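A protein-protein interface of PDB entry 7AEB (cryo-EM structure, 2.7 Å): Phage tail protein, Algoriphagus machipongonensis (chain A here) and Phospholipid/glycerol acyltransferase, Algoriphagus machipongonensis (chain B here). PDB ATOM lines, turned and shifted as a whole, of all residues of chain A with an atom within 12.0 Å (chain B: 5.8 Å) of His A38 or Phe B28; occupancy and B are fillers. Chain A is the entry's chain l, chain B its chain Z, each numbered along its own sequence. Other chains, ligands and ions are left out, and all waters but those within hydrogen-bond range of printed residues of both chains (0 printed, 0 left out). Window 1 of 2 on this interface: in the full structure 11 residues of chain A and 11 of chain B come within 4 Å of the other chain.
Glu B27 touches His A38.
His A38 touches Phe B28 (CA to O, 3.6 Å).
Tyr A44 touches Phe B10.
The backbone NH of Phe B12 is in hydrogen-bond range of the backbone carbonyl oxygen of Gly A39 (3.1 Å).
The backbone carbonyl oxygen (O) of Phe B10 lies within hydrogen-bond range of the guanidinium group (NH1) of Arg A37 (2.7 Å).
The backbone carbonyl oxygen of Phe B28 is in hydrogen-bond range of the backbone NH of Gly A39.
The backbone NH (N) of Ala A40 sits close to the backbone carbonyl oxygen (O) of Phe B12.
O of Phe B10 lies close to O of Gly A39, at 3.2 Å.
The backbone carbonyl oxygen (O) of Gly A39 is in hydrogen-bond range of the guanidinium group (NH2) of Arg A37 (3.3 Å).
The guanidinium group (NH2) of Arg A37 lies within hydrogen-bond range of the backbone carbonyl oxygen (O) of Ser A41, 3.0 Å away.
O of Glu A43 is in hydrogen-bond range of NE of Arg A37, at 2.9 Å.
Printed residues of chain A that touch a printed residue of chain B: Arg A37, His A38, Gly A39, Ala A40 and Tyr A44.
Hydrophobic or aromatic side chains of chain A that line the printed part of chain B: His A38, Ala A40 and Tyr A44.
Among the printed residues, no Asp or Glu carboxylate lies within 4 Å of a Lys or Arg side-chain nitrogen of the other chain.
Ile A34 touches none of the printed residues of chain B.
Glu A35 touches none of the printed residues of chain B.
Of the printed residues of chain B, Arg A37 touches Phe B10 (2.7 Å).
Of the printed residues of chain B, Gly A39 touches Phe B10 (3.2 Å), Phe B12 (3.1 Å) and Phe B28 (2.9 Å).
Of the printed residues of chain B, Tyr A44 touches Phe B10.
Phe B12 touches two residues of chain A.
Val B14 touches none of the printed residues of chain A.
No residue of chain A comes within 4 Å of Asp B25.
Glu B27 touches one residue of chain A.
Of chain A, only His A38 and Gly A39 come within 4 Å of Phe B28.
No residue of chain A comes within 4 Å of Gln B29.
Ser B30 touches none of the printed residues of chain A.
No residue of chain A comes within 4 Å of Leu B66.
No residue of chain A comes within 4 Å of Arg B68.
The nearest residue of chain B that does not touch His A38 is Gln B29 (4.7 Å).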
ATOM      1  N   ILE A  34      14.025   9.769   9.575  1.00  0.00           N
ATOM      2  CA  ILE A  34      12.736   9.675  10.238  1.00  0.00           C
ATOM      3  C   ILE A  34      11.627  10.057   9.249  1.00  0.00           C
ATOM      4  O   ILE A  34      11.670  11.126   8.639  1.00  0.00           O
ATOM      5  CB  ILE A  34      12.708  10.586  11.473  1.00  0.00           C
ATOM      6  CG1 ILE A  34      13.813  10.138  12.447  1.00  0.00           C
ATOM      7  CG2 ILE A  34      11.323  10.528  12.125  1.00  0.00           C
ATOM      8  CD1 ILE A  34      14.099  11.096  13.552  1.00  0.00           C
ATOM      9  N   GLU A  35      10.659   9.159   9.049  1.00  0.00           N
ATOM     10  CA  GLU A  35       9.577   9.376   8.075  1.00  0.00           C
ATOM     11  C   GLU A  35       8.211   9.667   8.720  1.00  0.00           C
ATOM     12  O   GLU A  35       7.896   9.117   9.775  1.00  0.00           O
ATOM     13  CB  GLU A  35       9.449   8.150   7.178  1.00  0.00           C
ATOM     14  CG  GLU A  35      10.676   7.831   6.356  1.00  0.00           C
ATOM     15  CD  GLU A  35      10.486   6.650   5.457  1.00  0.00           C
ATOM     16  OE1 GLU A  35       9.474   6.006   5.585  1.00  0.00           O
ATOM     17  OE2 GLU A  35      11.340   6.382   4.641  1.00  0.00           O
ATOM     18  N   TYR A  36       7.375  10.476   8.048  1.00  0.00           N
ATOM     19  CA  TYR A  36       6.025  10.799   8.557  1.00  0.00           C
ATOM     20  C   TYR A  36       4.930  11.113   7.512  1.00  0.00           C
ATOM     21  O   TYR A  36       5.190  11.733   6.482  1.00  0.00           O
ATOM     22  CB  TYR A  36       6.157  12.012   9.490  1.00  0.00           C
ATOM     23  CG  TYR A  36       4.886  12.505  10.149  1.00  0.00           C
ATOM     24  CD1 TYR A  36       4.438  11.931  11.313  1.00  0.00           C
ATOM     25  CD2 TYR A  36       4.169  13.543   9.580  1.00  0.00           C
ATOM     26  CE1 TYR A  36       3.292  12.393  11.908  1.00  0.00           C
ATOM     27  CE2 TYR A  36       3.026  13.997  10.171  1.00  0.00           C
ATOM     28  CZ  TYR A  36       2.587  13.432  11.329  1.00  0.00           C
ATOM     29  OH  TYR A  36       1.445  13.890  11.928  1.00  0.00           O
ATOM     30  N   ARG A  37       3.689  10.668   7.768  1.00  0.00           N
ATOM     31  CA  ARG A  37       2.537  11.064   6.940  1.00  0.00           C
ATOM     32  C   ARG A  37       1.231  11.170   7.734  1.00  0.00           C
ATOM     33  O   ARG A  37       0.829  10.222   8.403  1.00  0.00           O
ATOM     34  CB  ARG A  37       2.281  10.109   5.765  1.00  0.00           C
ATOM     35  CG  ARG A  37       1.055  10.512   4.914  1.00  0.00           C
ATOM     36  CD  ARG A  37       0.769   9.687   3.702  1.00  0.00           C
ATOM     37  NE  ARG A  37      -0.449  10.219   3.036  1.00  0.00           N
ATOM     38  CZ  ARG A  37      -1.740   9.859   3.335  1.00  0.00           C
ATOM     39  NH1 ARG A  37      -1.976   8.920   4.230  1.00  0.00           N
ATOM     40  NH2 ARG A  37      -2.783  10.448   2.754  1.00  0.00           N
ATOM     41  N   HIS A  38       0.539  12.298   7.637  1.00  0.00           N
ATOM     42  CA  HIS A  38      -0.764  12.451   8.297  1.00  0.00           C
ATOM     43  C   HIS A  38      -1.870  12.094   7.292  1.00  0.00           C
ATOM     44  O   HIS A  38      -1.786  12.450   6.139  1.00  0.00           O
ATOM     45  CB  HIS A  38      -0.963  13.801   8.997  1.00  0.00           C
ATOM     46  CG  HIS A  38      -0.944  14.986   8.087  1.00  0.00           C
ATOM     47  ND1 HIS A  38      -2.089  15.598   7.643  1.00  0.00           N
ATOM     48  CD2 HIS A  38       0.079  15.688   7.559  1.00  0.00           C
ATOM     49  CE1 HIS A  38      -1.776  16.602   6.854  1.00  0.00           C
ATOM     50  NE2 HIS A  38      -0.466  16.691   6.803  1.00  0.00           N
ATOM     51  N   GLY A  39      -2.889  11.377   7.757  1.00  0.00           N
ATOM     52  CA  GLY A  39      -3.966  10.822   6.944  1.00  0.00           C
ATOM     53  C   GLY A  39      -4.650  11.767   5.955  1.00  0.00           C
ATOM     54  O   GLY A  39      -5.124  11.316   4.912  1.00  0.00           O
ATOM     55  N   ALA A  40      -4.724  13.057   6.260  1.00  0.00           N
ATOM     56  CA  ALA A  40      -5.385  14.000   5.369  1.00  0.00           C
ATOM     57  C   ALA A  40      -4.516  14.530   4.226  1.00  0.00           C
ATOM     58  O   ALA A  40      -5.003  15.330   3.432  1.00  0.00           O
ATOM     59  CB  ALA A  40      -5.894  15.177   6.170  1.00  0.00           C
ATOM     60  N   SER A  41      -3.243  14.162   4.149  1.00  0.00           N
ATOM     61  CA  SER A  41      -2.396  14.705   3.093  1.00  0.00           C
ATOM     62  C   SER A  41      -2.823  14.277   1.673  1.00  0.00           C
ATOM     63  O   SER A  41      -3.108  13.102   1.446  1.00  0.00           O
ATOM     64  CB  SER A  41      -0.964  14.278   3.289  1.00  0.00           C
ATOM     65  OG  SER A  41      -0.169  14.721   2.213  1.00  0.00           O
ATOM     66  N   PRO A  42      -2.859  15.201   0.678  1.00  0.00           N
ATOM     67  CA  PRO A  42      -3.083  14.954  -0.745  1.00  0.00           C
ATOM     68  C   PRO A  42      -2.026  14.060  -1.401  1.00  0.00           C
ATOM     69  O   PRO A  42      -2.245  13.547  -2.493  1.00  0.00           O
ATOM     70  CB  PRO A  42      -3.012  16.359  -1.347  1.00  0.00           C
ATOM     71  CG  PRO A  42      -3.350  17.273  -0.240  1.00  0.00           C
ATOM     72  CD  PRO A  42      -2.806  16.632   1.003  1.00  0.00           C
ATOM     73  N   GLU A  43      -0.849  13.941  -0.787  1.00  0.00           N
ATOM     74  CA  GLU A  43       0.187  13.092  -1.354  1.00  0.00           C
ATOM     75  C   GLU A  43       0.174  11.778  -0.626  1.00  0.00           C
ATOM     76  O   GLU A  43      -0.029  11.733   0.587  1.00  0.00           O
ATOM     77  CB  GLU A  43       1.570  13.728  -1.293  1.00  0.00           C
ATOM     78  CG  GLU A  43       1.738  14.938  -2.163  1.00  0.00           C
ATOM     79  CD  GLU A  43       3.148  15.480  -2.152  1.00  0.00           C
ATOM     80  OE1 GLU A  43       3.907  15.073  -1.312  1.00  0.00           O
ATOM     81  OE2 GLU A  43       3.463  16.285  -2.991  1.00  0.00           O
ATOM     82  N   TYR A  44       0.488  10.714  -1.342  1.00  0.00           N
ATOM     83  CA  TYR A  44       0.441   9.383  -0.781  1.00  0.00           C
ATOM     84  C   TYR A  44       1.819   8.796  -0.525  1.00  0.00           C
ATOM     85  O   TYR A  44       2.053   7.607  -0.712  1.00  0.00           O
ATOM     86  CB  TYR A  44      -0.423   8.515  -1.679  1.00  0.00           C
ATOM     87  CG  TYR A  44      -1.784   9.185  -1.916  1.00  0.00           C
ATOM     88  CD1 TYR A  44      -2.175   9.499  -3.194  1.00  0.00           C
ATOM     89  CD2 TYR A  44      -2.595   9.549  -0.856  1.00  0.00           C
ATOM     90  CE1 TYR A  44      -3.359  10.144  -3.420  1.00  0.00           C
ATOM     91  CE2 TYR A  44      -3.774  10.204  -1.082  1.00  0.00           C
ATOM     92  CZ  TYR A  44      -4.156  10.498  -2.365  1.00  0.00           C
ATOM     93  OH  TYR A  44      -5.336  11.148  -2.602  1.00  0.00           O
ATOM     94  N   SER A  45       2.722   9.661  -0.098  1.00  0.00           N
ATOM     95  CA  SER A  45       4.094   9.332   0.235  1.00  0.00           C
ATOM     96  C   SER A  45       4.478  10.099   1.497  1.00  0.00           C
ATOM     97  O   SER A  45       3.719  10.943   1.975  1.00  0.00           O
ATOM     98  CB  SER A  45       5.008   9.667  -0.920  1.00  0.00           C
ATOM     99  OG  SER A  45       5.036  11.038  -1.147  1.00  0.00           O
ATOM    100  N   LYS A  46       5.630   9.780   2.074  1.00  0.00           N
ATOM    101  CA  LYS A  46       6.053  10.386   3.341  1.00  0.00           C
ATOM    102  C   LYS A  46       7.043  11.544   3.240  1.00  0.00           C
ATOM    103  O   LYS A  46       7.797  11.655   2.274  1.00  0.00           O
ATOM    104  CB  LYS A  46       6.644   9.284   4.207  1.00  0.00           C
ATOM    105  CG  LYS A  46       5.633   8.221   4.569  1.00  0.00           C
ATOM    106  CD  LYS A  46       6.225   7.138   5.382  1.00  0.00           C
ATOM    107  CE  LYS A  46       5.224   6.068   5.686  1.00  0.00           C
ATOM    108  NZ  LYS A  46       5.840   4.949   6.442  1.00  0.00           N
ATOM    109  N   ILE A  47       7.074  12.372   4.288  1.00  0.00           N
ATOM    110  CA  ILE A  47       8.037  13.465   4.411  1.00  0.00           C
ATOM    111  C   ILE A  47       9.216  12.980   5.246  1.00  0.00           C
ATOM    112  O   ILE A  47       9.048  12.185   6.173  1.00  0.00           O
ATOM    113  CB  ILE A  47       7.421  14.765   4.985  1.00  0.00           C
ATOM    114  CG1 ILE A  47       6.867  14.557   6.417  1.00  0.00           C
ATOM    115  CG2 ILE A  47       6.326  15.225   4.030  1.00  0.00           C
ATOM    116  CD1 ILE A  47       6.481  15.810   7.149  1.00  0.00           C
ATOM    117  N   LYS A  48      10.430  13.391   4.878  1.00  0.00           N
ATOM    118  CA  LYS A  48      11.625  12.897   5.566  1.00  0.00           C
ATOM    119  C   LYS A  48      12.466  13.947   6.297  1.00  0.00           C
ATOM    120  O   LYS A  48      12.676  15.044   5.785  1.00  0.00           O
ATOM    121  CB  LYS A  48      12.479  12.247   4.492  1.00  0.00           C
ATOM    122  CG  LYS A  48      11.774  11.112   3.813  1.00  0.00           C
ATOM    123  CD  LYS A  48      12.573  10.478   2.732  1.00  0.00           C
ATOM    124  CE  LYS A  48      11.758   9.389   2.065  1.00  0.00           C
ATOM    125  NZ  LYS A  48      12.491   8.739   0.964  1.00  0.00           N
ATOM    126  N   PHE B  10      -6.276   4.987   4.083  1.00  0.00           N
ATOM    127  CA  PHE B  10      -5.230   5.927   4.480  1.00  0.00           C
ATOM    128  C   PHE B  10      -5.498   7.405   4.170  1.00  0.00           C
ATOM    129  O   PHE B  10      -4.579   8.217   4.304  1.00  0.00           O
ATOM    130  CB  PHE B  10      -3.877   5.526   3.885  1.00  0.00           C
ATOM    131  CG  PHE B  10      -3.860   5.327   2.403  1.00  0.00           C
ATOM    132  CD1 PHE B  10      -3.740   6.395   1.540  1.00  0.00           C
ATOM    133  CD2 PHE B  10      -3.885   4.059   1.878  1.00  0.00           C
ATOM    134  CE1 PHE B  10      -3.687   6.198   0.195  1.00  0.00           C
ATOM    135  CE2 PHE B  10      -3.821   3.865   0.529  1.00  0.00           C
ATOM    136  CZ  PHE B  10      -3.724   4.938  -0.314  1.00  0.00           C
ATOM    137  N   PHE B  12      -8.124  10.486   5.193  1.00  0.00           N
ATOM    138  CA  PHE B  12      -9.211  10.890   6.087  1.00  0.00           C
ATOM    139  C   PHE B  12      -8.943  12.229   6.790  1.00  0.00           C
ATOM    140  O   PHE B  12      -7.800  12.668   6.902  1.00  0.00           O
ATOM    141  CB  PHE B  12      -9.450   9.796   7.136  1.00  0.00           C
ATOM    142  CG  PHE B  12      -8.219   9.461   7.958  1.00  0.00           C
ATOM    143  CD1 PHE B  12      -7.929  10.131   9.134  1.00  0.00           C
ATOM    144  CD2 PHE B  12      -7.351   8.471   7.548  1.00  0.00           C
ATOM    145  CE1 PHE B  12      -6.785   9.835   9.850  1.00  0.00           C
ATOM    146  CE2 PHE B  12      -6.226   8.168   8.277  1.00  0.00           C
ATOM    147  CZ  PHE B  12      -5.951   8.849   9.434  1.00  0.00           C
ATOM    148  N   VAL B  14     -10.219  14.790  10.420  1.00  0.00           N
ATOM    149  CA  VAL B  14     -10.934  14.903  11.703  1.00  0.00           C
ATOM    150  C   VAL B  14     -11.259  16.370  11.974  1.00  0.00           C
ATOM    151  O   VAL B  14     -10.350  17.197  12.043  1.00  0.00           O
ATOM    152  CB  VAL B  14     -10.110  14.319  12.863  1.00  0.00           C
ATOM    153  CG1 VAL B  14     -10.849  14.474  14.190  1.00  0.00           C
ATOM    154  CG2 VAL B  14      -9.783  12.865  12.591  1.00  0.00           C
ATOM    155  N   PHE B  16     -13.503  19.345  14.393  1.00  0.00           N
ATOM    156  CA  PHE B  16     -14.075  19.608  15.702  1.00  0.00           C
ATOM    157  C   PHE B  16     -15.035  20.785  15.618  1.00  0.00           C
ATOM    158  O   PHE B  16     -14.757  21.760  14.926  1.00  0.00           O
ATOM    159  CB  PHE B  16     -12.970  19.951  16.704  1.00  0.00           C
ATOM    160  CG  PHE B  16     -11.937  18.870  16.899  1.00  0.00           C
ATOM    161  CD1 PHE B  16     -10.877  18.722  16.021  1.00  0.00           C
ATOM    162  CD2 PHE B  16     -11.999  18.031  17.986  1.00  0.00           C
ATOM    163  CE1 PHE B  16      -9.943  17.749  16.207  1.00  0.00           C
ATOM    164  CE2 PHE B  16     -11.052  17.060  18.179  1.00  0.00           C
ATOM    165  CZ  PHE B  16     -10.029  16.918  17.286  1.00  0.00           C
ATOM    166  N   ASP B  25      -4.687  21.212  13.731  1.00  0.00           N
ATOM    167  CA  ASP B  25      -5.446  20.331  14.604  1.00  0.00           C
ATOM    168  C   ASP B  25      -6.380  19.410  13.829  1.00  0.00           C
ATOM    169  O   ASP B  25      -7.159  18.683  14.439  1.00  0.00           O
ATOM    170  CB  ASP B  25      -6.260  21.123  15.658  1.00  0.00           C
ATOM    171  CG  ASP B  25      -5.419  21.654  16.869  1.00  0.00           C
ATOM    172  OD1 ASP B  25      -4.557  20.941  17.392  1.00  0.00           O
ATOM    173  OD2 ASP B  25      -5.682  22.778  17.334  1.00  0.00           O
ATOM    174  N   HIS B  26      -6.352  19.438  12.504  1.00  0.00           N
ATOM    175  CA  HIS B  26      -7.199  18.540  11.740  1.00  0.00           C
ATOM    176  C   HIS B  26      -6.433  17.381  11.171  1.00  0.00           C
ATOM    177  O   HIS B  26      -7.023  16.559  10.485  1.00  0.00           O
ATOM    178  CB  HIS B  26      -7.879  19.264  10.592  1.00  0.00           C
ATOM    179  CG  HIS B  26      -8.807  20.342  11.028  1.00  0.00           C
ATOM    180  ND1 HIS B  26      -9.366  20.384  12.285  1.00  0.00           N
ATOM    181  CD2 HIS B  26      -9.288  21.416  10.362  1.00  0.00           C
ATOM    182  CE1 HIS B  26     -10.147  21.442  12.379  1.00  0.00           C
ATOM    183  NE2 HIS B  26     -10.117  22.086  11.227  1.00  0.00           N
ATOM    184  N   GLU B  27      -5.142  17.292  11.433  1.00  0.00           N
ATOM    185  CA  GLU B  27      -4.308  16.260  10.837  1.00  0.00           C
ATOM    186  C   GLU B  27      -3.859  15.221  11.853  1.00  0.00           C
ATOM    187  O   GLU B  27      -3.184  15.551  12.828  1.00  0.00           O
ATOM    188  CB  GLU B  27      -3.106  16.917  10.185  1.00  0.00           C
ATOM    189  CG  GLU B  27      -3.492  18.159   9.433  1.00  0.00           C
ATOM    190  CD  GLU B  27      -2.307  19.022   9.121  1.00  0.00           C
ATOM    191  OE1 GLU B  27      -1.228  18.752   9.686  1.00  0.00           O
ATOM    192  OE2 GLU B  27      -2.451  19.967   8.317  1.00  0.00           O
ATOM    193  N   PHE B  28      -4.181  13.959  11.589  1.00  0.00           N
ATOM    194  CA  PHE B  28      -3.852  12.890  12.513  1.00  0.00           C
ATOM    195  C   PHE B  28      -3.187  11.718  11.816  1.00  0.00           C
ATOM    196  O   PHE B  28      -3.361  11.488  10.625  1.00  0.00           O
ATOM    197  CB  PHE B  28      -5.092  12.436  13.268  1.00  0.00           C
ATOM    198  CG  PHE B  28      -5.524  13.403  14.317  1.00  0.00           C
ATOM    199  CD1 PHE B  28      -6.469  14.379  14.040  1.00  0.00           C
ATOM    200  CD2 PHE B  28      -4.953  13.368  15.567  1.00  0.00           C
ATOM    201  CE1 PHE B  28      -6.845  15.283  15.003  1.00  0.00           C
ATOM    202  CE2 PHE B  28      -5.325  14.267  16.527  1.00  0.00           C
ATOM    203  CZ  PHE B  28      -6.270  15.225  16.246  1.00  0.00           C
ATOM    204  N   GLN B  29      -2.346  11.039  12.592  1.00  0.00           N
ATOM    205  CA  GLN B  29      -1.676   9.811  12.170  1.00  0.00           C
ATOM    206  C   GLN B  29      -2.625   8.615  12.160  1.00  0.00           C
ATOM    207  O   GLN B  29      -2.539   7.760  11.263  1.00  0.00           O
ATOM    208  CB  GLN B  29      -0.491   9.534  13.096  1.00  0.00           C
ATOM    209  CG  GLN B  29       0.244   8.242  12.796  1.00  0.00           C
ATOM    210  CD  GLN B  29       1.385   7.975  13.749  1.00  0.00           C
ATOM    211  OE1 GLN B  29       1.684   8.786  14.620  1.00  0.00           O
ATOM    212  NE2 GLN B  29       2.034   6.827  13.586  1.00  0.00           N
ATOM    213  N   SER B  30      -3.529   8.535  13.154  1.00  0.00           N
ATOM    214  CA  SER B  30      -4.400   7.375  13.254  1.00  0.00           C
ATOM    215  C   SER B  30      -5.665   7.699  14.063  1.00  0.00           C
ATOM    216  O   SER B  30      -5.648   8.516  14.990  1.00  0.00           O
ATOM    217  CB  SER B  30      -3.659   6.224  13.911  1.00  0.00           C
ATOM    218  OG  SER B  30      -4.550   5.183  14.182  1.00  0.00           O
ATOM    219  N   VAL B  31      -6.765   7.028  13.700  1.00  0.00           N
ATOM    220  CA  VAL B  31      -8.075   7.160  14.352  1.00  0.00           C
ATOM    221  C   VAL B  31      -8.597   5.771  14.693  1.00  0.00           C
ATOM    222  O   VAL B  31      -8.586   4.898  13.832  1.00  0.00           O
ATOM    223  CB  VAL B  31      -9.123   7.822  13.438  1.00  0.00           C
ATOM    224  CG1 VAL B  31     -10.314   8.294  14.245  1.00  0.00           C
ATOM    225  CG2 VAL B  31      -8.553   8.896  12.609  1.00  0.00           C
ATOM    226  N   LEU B  66      -7.275   9.177  19.189  1.00  0.00           N
ATOM    227  CA  LEU B  66      -6.553   9.916  18.163  1.00  0.00           C
ATOM    228  C   LEU B  66      -5.048   9.990  18.439  1.00  0.00           C
ATOM    229  O   LEU B  66      -4.634  10.292  19.561  1.00  0.00           O
ATOM    230  CB  LEU B  66      -7.126  11.332  18.061  1.00  0.00           C
ATOM    231  CG  LEU B  66      -8.626  11.499  17.754  1.00  0.00           C
ATOM    232  CD1 LEU B  66      -9.022  12.952  17.859  1.00  0.00           C
ATOM    233  CD2 LEU B  66      -8.922  11.001  16.375  1.00  0.00           C
ATOM    234  N   LYS B  67      -4.219   9.783  17.405  1.00  0.00           N
ATOM    235  CA  LYS B  67      -2.765   9.920  17.539  1.00  0.00           C
ATOM    236  C   LYS B  67      -2.158  10.838  16.485  1.00  0.00           C
ATOM    237  O   LYS B  67      -2.637  10.903  15.350  1.00  0.00           O
ATOM    238  CB  LYS B  67      -2.056   8.580  17.444  1.00  0.00           C
ATOM    239  CG  LYS B  67      -2.345   7.658  18.575  1.00  0.00           C
ATOM    240  CD  LYS B  67      -1.552   6.390  18.440  1.00  0.00           C
ATOM    241  CE  LYS B  67      -1.829   5.445  19.588  1.00  0.00           C
ATOM    242  NZ  LYS B  67      -1.105   4.151  19.428  1.00  0.00           N
ATOM    243  N   ARG B  68      -1.062  11.510  16.865  1.00  0.00           N
ATOM    244  CA  ARG B  68      -0.304  12.405  15.987  1.00  0.00           C
ATOM    245  C   ARG B  68       1.063  12.737  16.585  1.00  0.00           C
ATOM    246  O   ARG B  68       1.319  12.465  17.756  1.00  0.00           O
ATOM    247  CB  ARG B  68      -1.057  13.699  15.760  1.00  0.00           C
ATOM    248  CG  ARG B  68      -1.200  14.490  17.020  1.00  0.00           C
ATOM    249  CD  ARG B  68      -1.907  15.734  16.774  1.00  0.00           C
ATOM    250  NE  ARG B  68      -1.915  16.528  17.978  1.00  0.00           N
ATOM    251  CZ  ARG B  68      -2.575  17.661  18.133  1.00  0.00           C
ATOM    252  NH1 ARG B  68      -3.320  18.164  17.160  1.00  0.00           N
ATOM    253  NH2 ARG B  68      -2.465  18.284  19.285  1.00  0.00           N
